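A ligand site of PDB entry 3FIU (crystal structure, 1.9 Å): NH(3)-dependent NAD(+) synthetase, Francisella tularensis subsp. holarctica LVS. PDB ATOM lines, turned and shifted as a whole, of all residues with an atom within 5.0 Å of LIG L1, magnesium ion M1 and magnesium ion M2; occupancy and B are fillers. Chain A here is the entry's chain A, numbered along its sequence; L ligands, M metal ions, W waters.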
ATOM      1  N   ILE A  34      -8.277  11.227 -19.010  1.00  0.00           N
ATOM      2  CA  ILE A  34      -7.768  12.575 -19.199  1.00  0.00           C
ATOM      3  C   ILE A  34      -7.342  12.753 -20.653  1.00  0.00           C
ATOM      4  O   ILE A  34      -6.817  11.815 -21.248  1.00  0.00           O
ATOM      5  CB  ILE A  34      -6.601  12.871 -18.244  1.00  0.00           C
ATOM      6  CG1 ILE A  34      -6.197  14.349 -18.356  1.00  0.00           C
ATOM      7  CG2 ILE A  34      -5.393  11.984 -18.552  1.00  0.00           C
ATOM      8  CD1 ILE A  34      -5.457  14.846 -17.153  1.00  0.00           C
ATOM      9  N   GLY A  35      -7.647  13.914 -21.242  1.00  0.00           N
ATOM     10  CA  GLY A  35      -7.140  14.235 -22.584  1.00  0.00           C
ATOM     11  C   GLY A  35      -5.735  14.830 -22.477  1.00  0.00           C
ATOM     12  O   GLY A  35      -5.508  15.805 -21.734  1.00  0.00           O
ATOM     13  N   LEU A  36      -4.780  14.234 -23.203  1.00  0.00           N
ATOM     14  CA  LEU A  36      -3.384  14.708 -23.173  1.00  0.00           C
ATOM     15  C   LEU A  36      -3.023  15.451 -24.440  1.00  0.00           C
ATOM     16  O   LEU A  36      -2.951  14.862 -25.525  1.00  0.00           O
ATOM     17  CB  LEU A  36      -2.393  13.551 -22.981  1.00  0.00           C
ATOM     18  CG  LEU A  36      -2.022  12.987 -21.627  1.00  0.00           C
ATOM     19  CD1 LEU A  36      -0.831  12.064 -21.874  1.00  0.00           C
ATOM     20  CD2 LEU A  36      -1.621  14.049 -20.628  1.00  0.00           C
ATOM     21  N   SER A  37      -2.782  16.753 -24.302  1.00  0.00           N
ATOM     22  CA  SER A  37      -2.513  17.624 -25.433  1.00  0.00           C
ATOM     23  C   SER A  37      -1.018  17.729 -25.748  1.00  0.00           C
ATOM     24  O   SER A  37      -0.652  18.206 -26.795  1.00  0.00           O
ATOM     25  CB  SER A  37      -3.013  19.019 -25.099  1.00  0.00           C
ATOM     26  OG  SER A  37      -2.305  19.491 -23.957  1.00  0.00           O
ATOM     27  N   GLY A  39       0.689  19.463 -23.673  1.00  0.00           N
ATOM     28  CA  GLY A  39       0.933  20.650 -22.794  1.00  0.00           C
ATOM     29  C   GLY A  39       1.175  20.285 -21.332  1.00  0.00           C
ATOM     30  O   GLY A  39       0.978  19.157 -20.908  1.00  0.00           O
ATOM     31  N   ASP A  41      -0.418  21.425 -18.425  1.00  0.00           N
ATOM     32  CA  ASP A  41      -1.570  21.264 -17.489  1.00  0.00           C
ATOM     33  C   ASP A  41      -2.042  19.822 -17.518  1.00  0.00           C
ATOM     34  O   ASP A  41      -2.219  19.202 -16.472  1.00  0.00           O
ATOM     35  CB  ASP A  41      -2.768  22.171 -17.863  1.00  0.00           C
ATOM     36  CG  ASP A  41      -2.453  23.663 -17.805  1.00  0.00           C
ATOM     37  OD1 ASP A  41      -1.601  24.082 -16.984  1.00  0.00           O
ATOM     38  OD2 ASP A  41      -3.099  24.410 -18.596  1.00  0.00           O
ATOM     39  N   SER A  42      -2.233  19.283 -18.725  1.00  0.00           N
ATOM     40  CA  SER A  42      -2.720  17.909 -18.823  1.00  0.00           C
ATOM     41  C   SER A  42      -1.622  16.920 -18.437  1.00  0.00           C
ATOM     42  O   SER A  42      -1.923  15.870 -17.842  1.00  0.00           O
ATOM     43  CB  SER A  42      -3.287  17.582 -20.204  1.00  0.00           C
ATOM     44  OG  SER A  42      -2.346  17.902 -21.229  1.00  0.00           O
ATOM     45  N   LEU A  59      -6.359   9.932 -23.406  1.00  0.00           N
ATOM     46  CA  LEU A  59      -6.751  10.019 -24.791  1.00  0.00           C
ATOM     47  C   LEU A  59      -5.928  11.118 -25.472  1.00  0.00           C
ATOM     48  O   LEU A  59      -5.842  12.229 -24.974  1.00  0.00           O
ATOM     49  CB  LEU A  59      -8.256  10.318 -24.921  1.00  0.00           C
ATOM     50  CG  LEU A  59      -9.208   9.355 -24.226  1.00  0.00           C
ATOM     51  CD1 LEU A  59     -10.664   9.697 -24.671  1.00  0.00           C
ATOM     52  CD2 LEU A  59      -8.835   7.909 -24.577  1.00  0.00           C
ATOM     53  N   ILE A  60      -5.326  10.777 -26.602  1.00  0.00           N
ATOM     54  CA  ILE A  60      -4.740  11.783 -27.477  1.00  0.00           C
ATOM     55  C   ILE A  60      -5.666  11.994 -28.649  1.00  0.00           C
ATOM     56  O   ILE A  60      -6.009  11.051 -29.370  1.00  0.00           O
ATOM     57  CB  ILE A  60      -3.347  11.380 -27.944  1.00  0.00           C
ATOM     58  CG1 ILE A  60      -2.438  11.143 -26.740  1.00  0.00           C
ATOM     59  CG2 ILE A  60      -2.739  12.428 -28.971  1.00  0.00           C
ATOM     60  CD1 ILE A  60      -1.056  10.613 -27.136  1.00  0.00           C
ATOM     61  N   LEU A  61      -6.055  13.254 -28.861  1.00  0.00           N
ATOM     62  CA  LEU A  61      -7.188  13.563 -29.744  1.00  0.00           C
ATOM     63  C   LEU A  61      -6.847  14.665 -30.727  1.00  0.00           C
ATOM     64  O   LEU A  61      -7.446  15.764 -30.694  1.00  0.00           O
ATOM     65  CB  LEU A  61      -8.434  13.934 -28.889  1.00  0.00           C
ATOM     66  CG  LEU A  61      -8.827  12.824 -27.921  1.00  0.00           C
ATOM     67  CD1 LEU A  61      -9.889  13.299 -26.897  1.00  0.00           C
ATOM     68  CD2 LEU A  61      -9.380  11.678 -28.769  1.00  0.00           C
ATOM     69  N   PRO A  62      -5.887  14.385 -31.627  1.00  0.00           N
ATOM     70  CA  PRO A  62      -5.475  15.447 -32.557  1.00  0.00           C
ATOM     71  C   PRO A  62      -6.511  15.801 -33.626  1.00  0.00           C
ATOM     72  O   PRO A  62      -7.254  14.939 -34.114  1.00  0.00           O
ATOM     73  CB  PRO A  62      -4.217  14.872 -33.199  1.00  0.00           C
ATOM     74  CG  PRO A  62      -4.328  13.398 -33.053  1.00  0.00           C
ATOM     75  CD  PRO A  62      -5.129  13.126 -31.838  1.00  0.00           C
ATOM     76  N   ASN A  66      -3.478  20.478 -35.132  1.00  0.00           N
ATOM     77  CA  ASN A  66      -2.484  20.190 -34.080  1.00  0.00           C
ATOM     78  C   ASN A  66      -1.109  19.859 -34.641  1.00  0.00           C
ATOM     79  O   ASN A  66      -0.988  19.343 -35.753  1.00  0.00           O
ATOM     80  CB  ASN A  66      -2.954  19.052 -33.167  1.00  0.00           C
ATOM     81  CG  ASN A  66      -4.093  19.461 -32.235  1.00  0.00           C
ATOM     82  OD1 ASN A  66      -3.908  20.198 -31.271  1.00  0.00           O
ATOM     83  ND2 ASN A  66      -5.267  18.975 -32.525  1.00  0.00           N
ATOM     84  N   ARG A 124     -13.678  16.668 -28.050  1.00  0.00           N
ATOM     85  CA  ARG A 124     -12.804  16.001 -27.080  1.00  0.00           C
ATOM     86  C   ARG A 124     -13.552  15.632 -25.799  1.00  0.00           C
ATOM     87  O   ARG A 124     -13.363  14.569 -25.276  1.00  0.00           O
ATOM     88  CB  ARG A 124     -11.565  16.871 -26.774  1.00  0.00           C
ATOM     89  CG  ARG A 124     -10.656  16.948 -28.023  1.00  0.00           C
ATOM     90  CD  ARG A 124      -9.224  17.468 -27.741  1.00  0.00           C
ATOM     91  NE  ARG A 124      -8.522  17.625 -29.018  1.00  0.00           N
ATOM     92  CZ  ARG A 124      -8.401  18.775 -29.678  1.00  0.00           C
ATOM     93  NH1 ARG A 124      -8.863  19.923 -29.186  1.00  0.00           N
ATOM     94  NH2 ARG A 124      -7.778  18.788 -30.853  1.00  0.00           N
ATOM     95  N   THR A 142      -8.413  19.985 -16.704  1.00  0.00           N
ATOM     96  CA  THR A 142      -7.032  20.424 -16.470  1.00  0.00           C
ATOM     97  C   THR A 142      -6.889  21.930 -16.210  1.00  0.00           C
ATOM     98  O   THR A 142      -5.774  22.428 -16.081  1.00  0.00           O
ATOM     99  CB  THR A 142      -6.127  20.069 -17.656  1.00  0.00           C
ATOM    100  OG1 THR A 142      -6.560  20.811 -18.781  1.00  0.00           O
ATOM    101  CG2 THR A 142      -6.151  18.555 -17.960  1.00  0.00           C
ATOM    102  N   ASN A 144      -6.302  25.454 -14.858  1.00  0.00           N
ATOM    103  CA  ASN A 144      -5.543  25.980 -13.732  1.00  0.00           C
ATOM    104  C   ASN A 144      -6.194  27.323 -13.332  1.00  0.00           C
ATOM    105  O   ASN A 144      -7.144  27.772 -14.016  1.00  0.00           O
ATOM    106  CB  ASN A 144      -4.045  26.138 -14.084  1.00  0.00           C
ATOM    107  CG  ASN A 144      -3.823  27.048 -15.275  1.00  0.00           C
ATOM    108  OD1 ASN A 144      -4.331  28.159 -15.322  1.00  0.00           O
ATOM    109  ND2 ASN A 144      -3.050  26.572 -16.267  1.00  0.00           N
ATOM    110  N   GLU A 147      -6.294  30.037 -16.391  1.00  0.00           N
ATOM    111  CA  GLU A 147      -7.335  29.736 -17.378  1.00  0.00           C
ATOM    112  C   GLU A 147      -8.723  29.966 -16.826  1.00  0.00           C
ATOM    113  O   GLU A 147      -9.568  30.590 -17.489  1.00  0.00           O
ATOM    114  CB  GLU A 147      -7.180  28.309 -17.886  1.00  0.00           C
ATOM    115  CG  GLU A 147      -5.797  28.036 -18.384  1.00  0.00           C
ATOM    116  CD  GLU A 147      -5.538  26.547 -18.643  1.00  0.00           C
ATOM    117  OE1 GLU A 147      -4.992  26.265 -19.710  1.00  0.00           O
ATOM    118  OE2 GLU A 147      -5.907  25.686 -17.825  1.00  0.00           O
ATOM    119  N   ASP A 158     -13.282  21.851 -22.883  1.00  0.00           N
ATOM    120  CA  ASP A 158     -12.275  21.548 -21.855  1.00  0.00           C
ATOM    121  C   ASP A 158     -12.678  22.114 -20.500  1.00  0.00           C
ATOM    122  O   ASP A 158     -12.194  21.653 -19.480  1.00  0.00           O
ATOM    123  CB  ASP A 158     -10.863  22.015 -22.292  1.00  0.00           C
ATOM    124  CG  ASP A 158     -10.808  23.503 -22.565  1.00  0.00           C
ATOM    125  OD1 ASP A 158      -9.941  24.147 -21.963  1.00  0.00           O
ATOM    126  OD2 ASP A 158     -11.627  24.006 -23.356  1.00  0.00           O
ATOM    127  N   LYS A 171      -0.029  29.365 -12.821  1.00  0.00           N
ATOM    128  CA  LYS A 171       0.688  28.640 -13.881  1.00  0.00           C
ATOM    129  C   LYS A 171       2.104  28.233 -13.434  1.00  0.00           C
ATOM    130  O   LYS A 171       2.567  27.122 -13.674  1.00  0.00           O
ATOM    131  CB  LYS A 171       0.710  29.476 -15.158  1.00  0.00           C
ATOM    132  CG  LYS A 171       1.193  28.716 -16.408  1.00  0.00           C
ATOM    133  CD  LYS A 171       0.116  27.705 -16.844  1.00  0.00           C
ATOM    134  CE  LYS A 171       0.545  26.984 -18.132  1.00  0.00           C
ATOM    135  NZ  LYS A 171      -0.604  26.089 -18.659  1.00  0.00           N
ATOM    136  N   SER A 193      -0.171  26.674 -25.103  1.00  0.00           N
ATOM    137  CA  SER A 193      -0.802  26.891 -26.399  1.00  0.00           C
ATOM    138  C   SER A 193      -2.075  26.074 -26.500  1.00  0.00           C
ATOM    139  O   SER A 193      -2.094  24.928 -26.038  1.00  0.00           O
ATOM    140  CB  SER A 193       0.150  26.496 -27.525  1.00  0.00           C
ATOM    141  OG  SER A 193      -0.509  26.537 -28.773  1.00  0.00           O
ATOM    142  N   ALA A 194      -3.111  26.627 -27.126  1.00  0.00           N
ATOM    143  CA  ALA A 194      -4.337  25.858 -27.344  1.00  0.00           C
ATOM    144  C   ALA A 194      -4.205  24.918 -28.552  1.00  0.00           C
ATOM    145  O   ALA A 194      -5.125  24.143 -28.830  1.00  0.00           O
ATOM    146  CB  ALA A 194      -5.589  26.812 -27.491  1.00  0.00           C
HETATM  147  P1  LIG L   1      -5.465  24.182 -23.582  1.00  0.00           P
HETATM  148  O1  LIG L   1      -5.456  24.737 -22.177  1.00  0.00           O
HETATM  149  O2  LIG L   1      -6.589  24.797 -24.443  1.00  0.00           O
HETATM  150  O3  LIG L   1      -4.177  24.064 -24.317  1.00  0.00           O
HETATM  151  O4  LIG L   1      -6.025  22.653 -23.460  1.00  0.00           O
HETATM  152  C1  LIG L   1      -7.110  22.382 -22.560  1.00  0.00           C
HETATM  153  C2  LIG L   1      -7.227  20.874 -22.389  1.00  0.00           C
HETATM  154  O5  LIG L   1      -7.843  20.264 -23.528  1.00  0.00           O
HETATM  155  C3  LIG L   1      -5.881  20.170 -22.302  1.00  0.00           C
HETATM  156  O6  LIG L   1      -5.385  20.297 -20.970  1.00  0.00           O
HETATM  157  C4  LIG L   1      -6.256  18.737 -22.657  1.00  0.00           C
HETATM  158  O7  LIG L   1      -6.758  18.023 -21.505  1.00  0.00           O
HETATM  159  C5  LIG L   1      -7.354  18.934 -23.692  1.00  0.00           C
HETATM  160  N1  LIG L   1      -6.759  18.846 -25.047  1.00  0.00           N
HETATM  161  C6  LIG L   1      -6.399  19.888 -25.853  1.00  0.00           C
HETATM  162  N2  LIG L   1      -5.871  19.434 -27.018  1.00  0.00           N
HETATM  163  C7  LIG L   1      -5.852  18.085 -26.946  1.00  0.00           C
HETATM  164  C8  LIG L   1      -5.435  16.983 -27.838  1.00  0.00           C
HETATM  165  N3  LIG L   1      -4.864  17.259 -29.036  1.00  0.00           N
HETATM  166  N4  LIG L   1      -5.634  15.737 -27.368  1.00  0.00           N
HETATM  167  C9  LIG L   1      -6.166  15.446 -26.168  1.00  0.00           C
HETATM  168  N5  LIG L   1      -6.597  16.397 -25.295  1.00  0.00           N
HETATM  169  C10 LIG L   1      -6.457  17.700 -25.656  1.00  0.00           C
HETATM  170  P1  LG2 L   2      -2.424  21.918 -21.727  1.00  0.00           P
HETATM  171  O1  LG2 L   2      -2.010  20.580 -21.158  1.00  0.00           O
HETATM  172  O2  LG2 L   2      -3.683  22.414 -21.081  1.00  0.00           O
HETATM  173  O3  LG2 L   2      -2.610  21.917 -23.238  1.00  0.00           O
HETATM  174  O4  LG2 L   2      -1.279  22.993 -21.321  1.00  0.00           O
HETATM  175  P2  LG2 L   2      -1.334  24.532 -21.795  1.00  0.00           P
HETATM  176  O5  LG2 L   2      -2.565  25.204 -21.196  1.00  0.00           O
HETATM  177  O6  LG2 L   2      -0.084  25.075 -21.160  1.00  0.00           O
HETATM  178  O7  LG2 L   2      -1.276  24.697 -23.291  1.00  0.00           O
HETATM  179 MG    MG M   1      -4.199  24.331 -20.397  1.00  0.00          MG
HETATM  180 MG    MG M   2      -2.354  23.371 -24.530  1.00  0.00          MG
HETATM  181  O   HOH W   1      -5.592  27.961 -22.199  1.00  0.00           O
HETATM  182  O   HOH W   2      -9.688  20.671 -26.504  1.00  0.00           O
HETATM  183  O   HOH W   3      -2.238  16.184 -30.372  1.00  0.00           O
HETATM  184  O   HOH W   4      -5.344  21.110 -29.227  1.00  0.00           O
HETATM  185  O   HOH W   5      -6.398  23.336 -26.366  1.00  0.00           O
HETATM  186  O   HOH W   6      -3.347  22.263 -26.050  1.00  0.00           O
HETATM  187  O   HOH W   7      -2.017  18.998 -29.071  1.00  0.00           O
HETATM  188  O   HOH W   8      -0.632  22.692 -25.349  1.00  0.00           O
HETATM  189  O   HOH W   9      -8.787  23.181 -19.637  1.00  0.00           O
HETATM  190  O   HOH W  10      -5.929  23.479 -19.253  1.00  0.00           O
HETATM  191  O   HOH W  11      -7.781  26.228 -21.982  1.00  0.00           O
HETATM  192  O   HOH W  12      -9.390  18.525 -20.713  1.00  0.00           O
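The backbone NH (N) of Leu 61 is in hydrogen-bond range of a nitrogen (N4) of LIG L1 (2.9 Å).
An oxygen (O7) of LG2 L2 sits close to the backbone NH of Ser 193, at 2.9 Å.
O1 of LG2 L2 is in hydrogen-bond range of N of Asp 41 (3.3 Å).
O6 of LG2 L2 lies within salt-bridge range of NZ of Lys 171 (2.7 Å).
A nitrogen (N3) of LIG L1 lies within hydrogen-bond range of the backbone carbonyl oxygen (O) of Leu 61, at 3.4 Å.
O1 of LG2 L2 is in hydrogen-bond range of OG of Ser 37 (3.0 Å).
An oxygen (O1) of LG2 L2 sits at hydrogen-bond distance from the backbone NH of Ser 42 (2.8 Å).
O of Gly 35 sits at hydrogen-bond distance from O7 of LIG L1 (2.6 Å).
O6 of LIG L1 is in hydrogen-bond range of OG1 of Thr 142 (2.5 Å).
The side-chain hydroxyl of Ser 42 sits at hydrogen-bond distance from an oxygen (O1) of LG2 L2 (2.7 Å).
The side-chain hydroxyl (OG) of Ser 37 sits at hydrogen-bond distance from the side-chain hydroxyl (OG) of Ser 42 (3.2 Å).
The backbone NH (N) of Glu 147 is in hydrogen-bond range of the side-chain amide oxygen (OD1) of Asn 144, at 2.9 Å.
The backbone NH (N) of Gly 39 lies within hydrogen-bond range of the side-chain hydroxyl (OG) of Ser 37 (3.0 Å).
NZ of Lys 171 lies within salt-bridge range of OD1 of Asp 41 (2.8 Å).
O of Ile 34 is in hydrogen-bond range of N of Leu 59, 2.9 Å away.
The guanidinium group (NE) of Arg 124 lies within hydrogen-bond range of the backbone carbonyl oxygen (O) of Leu 61 (2.7 Å).
ND2 of Asn 66 lies close to NH2 of Arg 124 (3.0 Å).
OD1 of Asp 41 lies within hydrogen-bond range of ND2 of Asn 144, 3.0 Å away.
The backbone carbonyl oxygen (O) of Leu 36 sits close to a nitrogen (N4) of LIG L1 (3.4 Å).
CB of Ser 37 touches N2 of LIG L1, 3.5 Å away.
Ser 42 touches LIG L1 (CB to O6, 3.5 Å).
Leu 59 touches LIG L1 (O to C9, 3.4 Å).
Ile 60 touches LIG L1 (C to N4, 3.96 Å).
Asn 66 touches LIG L1.
Arg 124 touches LIG L1 (NE to C8, 3.4 Å).
Asp 158 touches LIG L1.
Ala 194 touches LIG L1 (CA to O3, 3.5 Å).
Hydrophobic or aromatic side chains within 4 Å of LIG L1: Leu 61 and Ala 194.
Within 4 Å of LIG L1: Gly 35, Leu 36, Ser 37, Ser 42, Leu 59, Ile 60, Leu 61, Asn 66, Arg 124, Thr 142, Glu 147, Asp 158, Ser 193 and Ala 194.
The nearest printed residue that does not touch LIG L1 is Pro 62 (4.002 Å).
Of the 20 residues printed, 2 come within 4 Å of magnesium ion M1.
The nearest printed residue that does not touch magnesium ion M1 is Lys 171 (4.4 Å).
Residues that only touch magnesium ion M2: Ser 37.
Within 4 Å of magnesium ion M2: Ser 37 and Ser 193.
Magnesium ion M1 is bound by O5 of LG2 L2, at 2.0 Å.
Magnesium ion M1 is bound by O2 of LG2 L2 (2.1 Å).
Magnesium ion M1 is bound by OD2 of Asp 41 (2.1 Å).
Magnesium ion M1 is bound by the side-chain carboxylate (OE1) of Glu 147, at 2.2 Å.
O1 of LIG L1 is bound to magnesium ion M1 (2.2 Å).
Magnesium ion M1 is bound by water W10 (2.2 Å).
Magnesium ion M1 has six donor atoms within binding distance.
Magnesium ion M2 is bound by an oxygen (O3) of LIG L1, 2.0 Å away.
O3 of LG2 L2 binds magnesium ion M2.
Magnesium ion M2 is bound by water W8, at 2.0 Å.
Magnesium ion M2 is bound by an oxygen (O7) of LG2 L2.
Water W6 binds magnesium ion M2, at 2.1 Å.
Magnesium ion M2 is bound by the backbone carbonyl oxygen (O) of Ser 193.
Magnesium ion M2 has six donor atoms within binding distance.
Water W10 bridges the side-chain carboxylate of Glu 147 (2.6 Å) and the side-chain hydroxyl of Thr 142 (2.8 Å).
Water W5 bridges an oxygen (O2) of LIG L1 (2.4 Å) and the backbone carbonyl oxygen (O) of Ala 194 (2.9 Å).
Water W11 lies within hydrogen-bond range of the side-chain carboxylate of Asp 158 (3.0 Å) and an oxygen (O2) of LIG L1 (3.1 Å).
Water W7 lies within hydrogen-bond range of O of Ser 37 (2.8 Å), OD1 of Asn 66 (3.1 Å) and N3 of LIG L1 (3.3 Å).
Water W9 bridges the side-chain carboxylate (OD1) of Asp 158 and the side-chain hydroxyl (OG1) of Thr 142.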
